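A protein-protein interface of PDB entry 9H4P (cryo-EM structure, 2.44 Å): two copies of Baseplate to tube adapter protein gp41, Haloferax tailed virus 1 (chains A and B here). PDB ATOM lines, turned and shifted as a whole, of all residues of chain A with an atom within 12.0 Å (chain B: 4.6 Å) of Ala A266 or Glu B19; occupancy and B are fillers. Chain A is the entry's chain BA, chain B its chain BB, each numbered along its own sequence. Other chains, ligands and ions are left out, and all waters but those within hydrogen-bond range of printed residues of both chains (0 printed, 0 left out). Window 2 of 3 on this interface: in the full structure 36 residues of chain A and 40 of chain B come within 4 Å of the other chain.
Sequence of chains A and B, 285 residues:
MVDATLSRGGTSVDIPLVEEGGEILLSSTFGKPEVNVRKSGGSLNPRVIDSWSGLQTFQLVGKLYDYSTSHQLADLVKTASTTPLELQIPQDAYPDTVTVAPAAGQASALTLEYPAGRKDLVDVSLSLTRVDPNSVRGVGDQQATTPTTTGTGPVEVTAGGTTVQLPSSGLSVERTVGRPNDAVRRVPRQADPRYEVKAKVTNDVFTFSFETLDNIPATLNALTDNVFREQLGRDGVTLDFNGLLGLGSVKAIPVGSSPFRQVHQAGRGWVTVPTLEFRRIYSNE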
ATOM      1  N   GLU A 211       0.960  -6.456 -27.957  1.00  0.00           N
ATOM      2  CA  GLU A 211       0.602  -6.518 -26.544  1.00  0.00           C
ATOM      3  C   GLU A 211       1.878  -6.509 -25.694  1.00  0.00           C
ATOM      4  O   GLU A 211       2.781  -7.316 -25.929  1.00  0.00           O
ATOM      5  CB  GLU A 211      -0.336  -7.703 -26.280  1.00  0.00           C
ATOM      6  CG  GLU A 211      -1.581  -7.666 -27.157  1.00  0.00           C
ATOM      7  CD  GLU A 211      -2.756  -8.539 -26.756  1.00  0.00           C
ATOM      8  OE1 GLU A 211      -2.940  -8.780 -25.555  1.00  0.00           O
ATOM      9  OE2 GLU A 211      -3.483  -8.984 -27.656  1.00  0.00           O
ATOM     10  N   GLN A 262      -2.858   3.198 -25.366  1.00  0.00           N
ATOM     11  CA  GLN A 262      -2.591   2.177 -24.355  1.00  0.00           C
ATOM     12  C   GLN A 262      -3.925   1.724 -23.762  1.00  0.00           C
ATOM     13  O   GLN A 262      -4.643   2.537 -23.174  1.00  0.00           O
ATOM     14  CB  GLN A 262      -1.720   2.737 -23.222  1.00  0.00           C
ATOM     15  CG  GLN A 262      -0.321   3.180 -23.646  1.00  0.00           C
ATOM     16  CD  GLN A 262       0.504   3.865 -22.577  1.00  0.00           C
ATOM     17  OE1 GLN A 262       1.664   4.212 -22.801  1.00  0.00           O
ATOM     18  NE2 GLN A 262      -0.074   4.069 -21.402  1.00  0.00           N
ATOM     19  N   VAL A 263      -4.246   0.428 -23.910  1.00  0.00           N
ATOM     20  CA  VAL A 263      -5.557  -0.098 -23.538  1.00  0.00           C
ATOM     21  C   VAL A 263      -5.415  -1.135 -22.419  1.00  0.00           C
ATOM     22  O   VAL A 263      -4.662  -2.103 -22.546  1.00  0.00           O
ATOM     23  CB  VAL A 263      -6.343  -0.622 -24.766  1.00  0.00           C
ATOM     24  CG1 VAL A 263      -7.540  -1.495 -24.394  1.00  0.00           C
ATOM     25  CG2 VAL A 263      -6.804   0.525 -25.662  1.00  0.00           C
ATOM     26  N   HIS A 264      -6.179  -0.912 -21.339  1.00  0.00           N
ATOM     27  CA  HIS A 264      -6.203  -1.745 -20.143  1.00  0.00           C
ATOM     28  C   HIS A 264      -7.573  -2.412 -20.039  1.00  0.00           C
ATOM     29  O   HIS A 264      -8.597  -1.723 -20.040  1.00  0.00           O
ATOM     30  CB  HIS A 264      -5.925  -0.869 -18.906  1.00  0.00           C
ATOM     31  CG  HIS A 264      -4.584  -0.207 -18.929  1.00  0.00           C
ATOM     32  ND1 HIS A 264      -4.259   0.820 -19.810  1.00  0.00           N
ATOM     33  CD2 HIS A 264      -3.474  -0.445 -18.197  1.00  0.00           C
ATOM     34  CE1 HIS A 264      -3.004   1.183 -19.612  1.00  0.00           C
ATOM     35  NE2 HIS A 264      -2.505   0.428 -18.620  1.00  0.00           N
ATOM     36  N   GLN A 265      -7.583  -3.750 -19.945  1.00  0.00           N
ATOM     37  CA  GLN A 265      -8.829  -4.501 -19.888  1.00  0.00           C
ATOM     38  C   GLN A 265      -8.988  -5.140 -18.510  1.00  0.00           C
ATOM     39  O   GLN A 265      -7.994  -5.537 -17.895  1.00  0.00           O
ATOM     40  CB  GLN A 265      -8.891  -5.540 -21.010  1.00  0.00           C
ATOM     41  CG  GLN A 265      -9.124  -4.914 -22.381  1.00  0.00           C
ATOM     42  CD  GLN A 265      -9.047  -5.910 -23.512  1.00  0.00           C
ATOM     43  OE1 GLN A 265      -8.116  -5.891 -24.316  1.00  0.00           O
ATOM     44  NE2 GLN A 265     -10.039  -6.784 -23.595  1.00  0.00           N
ATOM     45  N   ALA A 266     -10.247  -5.226 -18.049  1.00  0.00           N
ATOM     46  CA  ALA A 266     -10.598  -5.844 -16.776  1.00  0.00           C
ATOM     47  C   ALA A 266     -10.017  -7.259 -16.695  1.00  0.00           C
ATOM     48  O   ALA A 266     -10.177  -8.048 -17.629  1.00  0.00           O
ATOM     49  CB  ALA A 266     -12.103  -5.845 -16.601  1.00  0.00           C
ATOM     50  N   GLY A 267      -9.308  -7.557 -15.595  1.00  0.00           N
ATOM     51  CA  GLY A 267      -8.808  -8.896 -15.304  1.00  0.00           C
ATOM     52  C   GLY A 267      -7.505  -9.280 -16.017  1.00  0.00           C
ATOM     53  O   GLY A 267      -7.070 -10.424 -15.883  1.00  0.00           O
ATOM     54  N   ARG A 268      -6.876  -8.346 -16.757  1.00  0.00           N
ATOM     55  CA  ARG A 268      -5.654  -8.630 -17.507  1.00  0.00           C
ATOM     56  C   ARG A 268      -4.465  -7.908 -16.872  1.00  0.00           C
ATOM     57  O   ARG A 268      -4.550  -6.714 -16.566  1.00  0.00           O
ATOM     58  CB  ARG A 268      -5.787  -8.230 -18.983  1.00  0.00           C
ATOM     59  CG  ARG A 268      -6.934  -8.917 -19.712  1.00  0.00           C
ATOM     60  CD  ARG A 268      -6.801  -8.875 -21.221  1.00  0.00           C
ATOM     61  NE  ARG A 268      -7.937  -9.559 -21.830  1.00  0.00           N
ATOM     62  CZ  ARG A 268      -8.082  -9.836 -23.124  1.00  0.00           C
ATOM     63  NH1 ARG A 268      -9.168 -10.464 -23.537  1.00  0.00           N
ATOM     64  NH2 ARG A 268      -7.153  -9.497 -24.001  1.00  0.00           N
ATOM     65  N   GLY A 269      -3.350  -8.642 -16.716  1.00  0.00           N
ATOM     66  CA  GLY A 269      -2.139  -8.131 -16.088  1.00  0.00           C
ATOM     67  C   GLY A 269      -1.147  -7.477 -17.055  1.00  0.00           C
ATOM     68  O   GLY A 269       0.044  -7.424 -16.744  1.00  0.00           O
ATOM     69  N   TRP A 270      -1.630  -6.970 -18.206  1.00  0.00           N
ATOM     70  CA  TRP A 270      -0.771  -6.398 -19.241  1.00  0.00           C
ATOM     71  C   TRP A 270      -1.531  -5.367 -20.086  1.00  0.00           C
ATOM     72  O   TRP A 270      -2.759  -5.284 -20.015  1.00  0.00           O
ATOM     73  CB  TRP A 270      -0.155  -7.519 -20.099  1.00  0.00           C
ATOM     74  CG  TRP A 270      -1.107  -8.146 -21.075  1.00  0.00           C
ATOM     75  CD1 TRP A 270      -1.374  -7.705 -22.340  1.00  0.00           C
ATOM     76  CD2 TRP A 270      -1.915  -9.331 -20.884  1.00  0.00           C
ATOM     77  NE1 TRP A 270      -2.289  -8.527 -22.943  1.00  0.00           N
ATOM     78  CE2 TRP A 270      -2.640  -9.538 -22.082  1.00  0.00           C
ATOM     79  CE3 TRP A 270      -2.099 -10.243 -19.832  1.00  0.00           C
ATOM     80  CZ2 TRP A 270      -3.526 -10.613 -22.244  1.00  0.00           C
ATOM     81  CZ3 TRP A 270      -2.976 -11.300 -19.990  1.00  0.00           C
ATOM     82  CH2 TRP A 270      -3.680 -11.485 -21.185  1.00  0.00           C
ATOM     83  N   VAL A 271      -0.785  -4.611 -20.909  1.00  0.00           N
ATOM     84  CA  VAL A 271      -1.328  -3.510 -21.695  1.00  0.00           C
ATOM     85  C   VAL A 271      -1.397  -3.939 -23.165  1.00  0.00           C
ATOM     86  O   VAL A 271      -0.435  -4.506 -23.694  1.00  0.00           O
ATOM     87  CB  VAL A 271      -0.501  -2.215 -21.492  1.00  0.00           C
ATOM     88  CG1 VAL A 271      -1.010  -1.041 -22.329  1.00  0.00           C
ATOM     89  CG2 VAL A 271      -0.410  -1.809 -20.024  1.00  0.00           C
ATOM     90  N   THR A 272      -2.551  -3.684 -23.803  1.00  0.00           N
ATOM     91  CA  THR A 272      -2.711  -3.812 -25.247  1.00  0.00           C
ATOM     92  C   THR A 272      -2.384  -2.471 -25.910  1.00  0.00           C
ATOM     93  O   THR A 272      -2.746  -1.416 -25.385  1.00  0.00           O
ATOM     94  CB  THR A 272      -4.145  -4.243 -25.600  1.00  0.00           C
ATOM     95  OG1 THR A 272      -4.440  -5.469 -24.926  1.00  0.00           O
ATOM     96  CG2 THR A 272      -4.398  -4.410 -27.084  1.00  0.00           C
ATOM     97  N   LEU B  17     -13.071   1.577 -10.981  1.00  0.00           N
ATOM     98  CA  LEU B  17     -12.484   0.994 -12.190  1.00  0.00           C
ATOM     99  C   LEU B  17     -12.610  -0.533 -12.185  1.00  0.00           C
ATOM    100  O   LEU B  17     -11.613  -1.258 -12.254  1.00  0.00           O
ATOM    101  CB  LEU B  17     -11.027   1.445 -12.386  1.00  0.00           C
ATOM    102  CG  LEU B  17     -10.788   2.919 -12.735  1.00  0.00           C
ATOM    103  CD1 LEU B  17      -9.346   3.158 -13.173  1.00  0.00           C
ATOM    104  CD2 LEU B  17     -11.746   3.430 -13.807  1.00  0.00           C
ATOM    105  N   VAL B  18     -13.865  -0.996 -12.097  1.00  0.00           N
ATOM    106  CA  VAL B  18     -14.212  -2.408 -12.184  1.00  0.00           C
ATOM    107  C   VAL B  18     -15.211  -2.585 -13.330  1.00  0.00           C
ATOM    108  O   VAL B  18     -16.056  -1.712 -13.560  1.00  0.00           O
ATOM    109  CB  VAL B  18     -14.750  -2.980 -10.846  1.00  0.00           C
ATOM    110  CG1 VAL B  18     -13.816  -2.750  -9.662  1.00  0.00           C
ATOM    111  CG2 VAL B  18     -16.162  -2.516 -10.501  1.00  0.00           C
ATOM    112  N   GLU B  19     -15.097  -3.713 -14.049  1.00  0.00           N
ATOM    113  CA  GLU B  19     -16.031  -4.045 -15.117  1.00  0.00           C
ATOM    114  C   GLU B  19     -16.188  -5.558 -15.263  1.00  0.00           C
ATOM    115  O   GLU B  19     -15.343  -6.328 -14.803  1.00  0.00           O
ATOM    116  CB  GLU B  19     -15.621  -3.424 -16.460  1.00  0.00           C
ATOM    117  CG  GLU B  19     -16.422  -2.185 -16.844  1.00  0.00           C
ATOM    118  CD  GLU B  19     -17.937  -2.305 -16.821  1.00  0.00           C
ATOM    119  OE1 GLU B  19     -18.465  -3.437 -16.883  1.00  0.00           O
ATOM    120  OE2 GLU B  19     -18.593  -1.256 -16.746  1.00  0.00           O
ATOM    121  N   GLU B  20     -17.282  -5.951 -15.934  1.00  0.00           N
ATOM    122  CA  GLU B  20     -17.589  -7.325 -16.304  1.00  0.00           C
ATOM    123  C   GLU B  20     -16.491  -7.901 -17.206  1.00  0.00           C
ATOM    124  O   GLU B  20     -16.038  -7.231 -18.138  1.00  0.00           O
ATOM    125  CB  GLU B  20     -18.918  -7.332 -17.065  1.00  0.00           C
ATOM    126  CG  GLU B  20     -19.479  -8.717 -17.326  1.00  0.00           C
ATOM    127  CD  GLU B  20     -20.412  -9.210 -16.240  1.00  0.00           C
ATOM    128  OE1 GLU B  20     -21.546  -8.714 -16.170  1.00  0.00           O
ATOM    129  OE2 GLU B  20     -19.995 -10.079 -15.461  1.00  0.00           O
ATOM    130  N   GLY B  21     -16.094  -9.151 -16.919  1.00  0.00           N
ATOM    131  CA  GLY B  21     -15.289  -9.974 -17.813  1.00  0.00           C
ATOM    132  C   GLY B  21     -13.984  -9.310 -18.260  1.00  0.00           C
ATOM    133  O   GLY B  21     -13.093  -9.078 -17.440  1.00  0.00           O
ATOM    134  N   GLY B  22     -13.890  -9.013 -19.569  1.00  0.00           N
ATOM    135  CA  GLY B  22     -12.693  -8.442 -20.174  1.00  0.00           C
ATOM    136  C   GLY B  22     -12.914  -7.103 -20.889  1.00  0.00           C
ATOM    137  O   GLY B  22     -12.218  -6.818 -21.864  1.00  0.00           O
ATOM    138  N   GLU B  23     -13.845  -6.273 -20.386  1.00  0.00           N
ATOM    139  CA  GLU B  23     -14.140  -4.967 -20.977  1.00  0.00           C
ATOM    140  C   GLU B  23     -12.993  -3.976 -20.737  1.00  0.00           C
ATOM    141  O   GLU B  23     -12.208  -4.162 -19.806  1.00  0.00           O
ATOM    142  CB  GLU B  23     -15.471  -4.420 -20.450  1.00  0.00           C
ATOM    143  CG  GLU B  23     -16.677  -4.889 -21.241  1.00  0.00           C
ATOM    144  CD  GLU B  23     -16.720  -4.452 -22.693  1.00  0.00           C
ATOM    145  OE1 GLU B  23     -16.031  -3.486 -23.050  1.00  0.00           O
ATOM    146  OE2 GLU B  23     -17.457  -5.081 -23.463  1.00  0.00           O
ATOM    147  N   LEU B  25     -11.259  -0.931 -19.297  1.00  0.00           N
ATOM    148  CA  LEU B  25     -11.373  -0.091 -18.109  1.00  0.00           C
ATOM    149  C   LEU B  25     -10.747   1.280 -18.341  1.00  0.00           C
ATOM    150  O   LEU B  25     -11.322   2.293 -17.940  1.00  0.00           O
ATOM    151  CB  LEU B  25     -10.705  -0.789 -16.921  1.00  0.00           C
ATOM    152  CG  LEU B  25     -11.530  -1.909 -16.291  1.00  0.00           C
ATOM    153  CD1 LEU B  25     -10.720  -2.657 -15.253  1.00  0.00           C
ATOM    154  CD2 LEU B  25     -12.796  -1.359 -15.656  1.00  0.00           C
ATOM    155  N   VAL B  61     -13.601   3.821 -17.626  1.00  0.00           N
ATOM    156  CA  VAL B  61     -14.881   3.143 -17.465  1.00  0.00           C
ATOM    157  C   VAL B  61     -14.876   2.462 -16.094  1.00  0.00           C
ATOM    158  O   VAL B  61     -13.911   1.775 -15.747  1.00  0.00           O
ATOM    159  CB  VAL B  61     -15.151   2.139 -18.614  1.00  0.00           C
ATOM    160  CG1 VAL B  61     -16.461   1.372 -18.441  1.00  0.00           C
ATOM    161  CG2 VAL B  61     -15.096   2.790 -19.994  1.00  0.00           C
ATOM    162  N   GLY B  62     -15.953   2.659 -15.324  1.00  0.00           N
ATOM    163  CA  GLY B  62     -16.070   2.029 -14.019  1.00  0.00           C
ATOM    164  C   GLY B  62     -17.510   2.028 -13.511  1.00  0.00           C
ATOM    165  O   GLY B  62     -18.432   2.392 -14.244  1.00  0.00           O
ATOM    166  N   LYS B  63     -17.678   1.623 -12.245  1.00  0.00           N
ATOM    167  CA  LYS B  63     -18.977   1.575 -11.585  1.00  0.00           C
ATOM    168  C   LYS B  63     -18.901   2.259 -10.222  1.00  0.00           C
ATOM    169  O   LYS B  63     -17.877   2.161  -9.548  1.00  0.00           O
ATOM    170  CB  LYS B  63     -19.436   0.121 -11.426  1.00  0.00           C
ATOM    171  CG  LYS B  63     -20.122  -0.464 -12.653  1.00  0.00           C
ATOM    172  CD  LYS B  63     -19.862  -1.950 -12.874  1.00  0.00           C
ATOM    173  CE  LYS B  63     -20.793  -2.581 -13.892  1.00  0.00           C
ATOM    174  NZ  LYS B  63     -20.782  -1.879 -15.200  1.00  0.00           N
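OE2 of Glu B19 lies within salt-bridge range of NZ of Lys B63, 2.8 Å away. The backbone NH of Val B61 is in hydrogen-bond range of the backbone carbonyl oxygen of Leu B25, at 2.8 Å.
Printed residues of chain B within 4 Å of His A264: Leu B25 (2.9 Å). Of the printed residues of chain B, Gln A265 touches Gly B22 (2.8 Å) and Glu B23 (3.4 Å). Ala A266 touches just these residues of chain B: Glu B19, Gly B21, Gly B22, Glu B23 and Leu B25. Of chain A, only Ala A266 comes within 4 Å of Glu B19. No residue of chain A comes within 4 Å of Glu B20. Gly B21 touches just one residue of chain A: Ala A266. Gly B22 touches just these residues of chain A: Gln A265 (2.8 Å) and Ala A266 (3.6 Å). Of chain A, only Gln A265 (3.4 Å) and Ala A266 (2.8 Å) come within 4 Å of Glu B23. No residue of chain A comes within 4 Å of Lys B63. The nearest residue of chain A that does not touch Glu B19 is Gly A267 (6.2 Å).
The backbone NH (N) of Leu B25 is in hydrogen-bond range of the backbone carbonyl oxygen (O) of His A264 (2.9 Å). O of Ala A266 lies close to O of Gly B21 (3.1 Å). N of Ala A266 lies within hydrogen-bond range of O of Glu B23 (2.8 Å). O of Gly B22 is in hydrogen-bond range of NE2 of Gln A265 (2.8 Å).
O of Glu B23 touches CA of Gln A265 (3.4 Å). CB of Ala A266 touches O of Glu B19, 3.7 Å away. Gly B22 touches Ala A266. CD1 of Leu B25 touches CA of Ala A266 (3.5 Å).
No position is printed for both chains.
Of the 12 printed residues of chain A, 3 touch a printed residue of chain B. Hydrophobic or aromatic side chains of chain A that line the printed part of chain B: Ala A266. Of the 11 printed residues of chain B, 5 touch a printed residue of chain A. Among the printed residues, no Asp or Glu carboxylate lies within 4 Å of a Lys or Arg side-chain nitrogen of the other chain.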
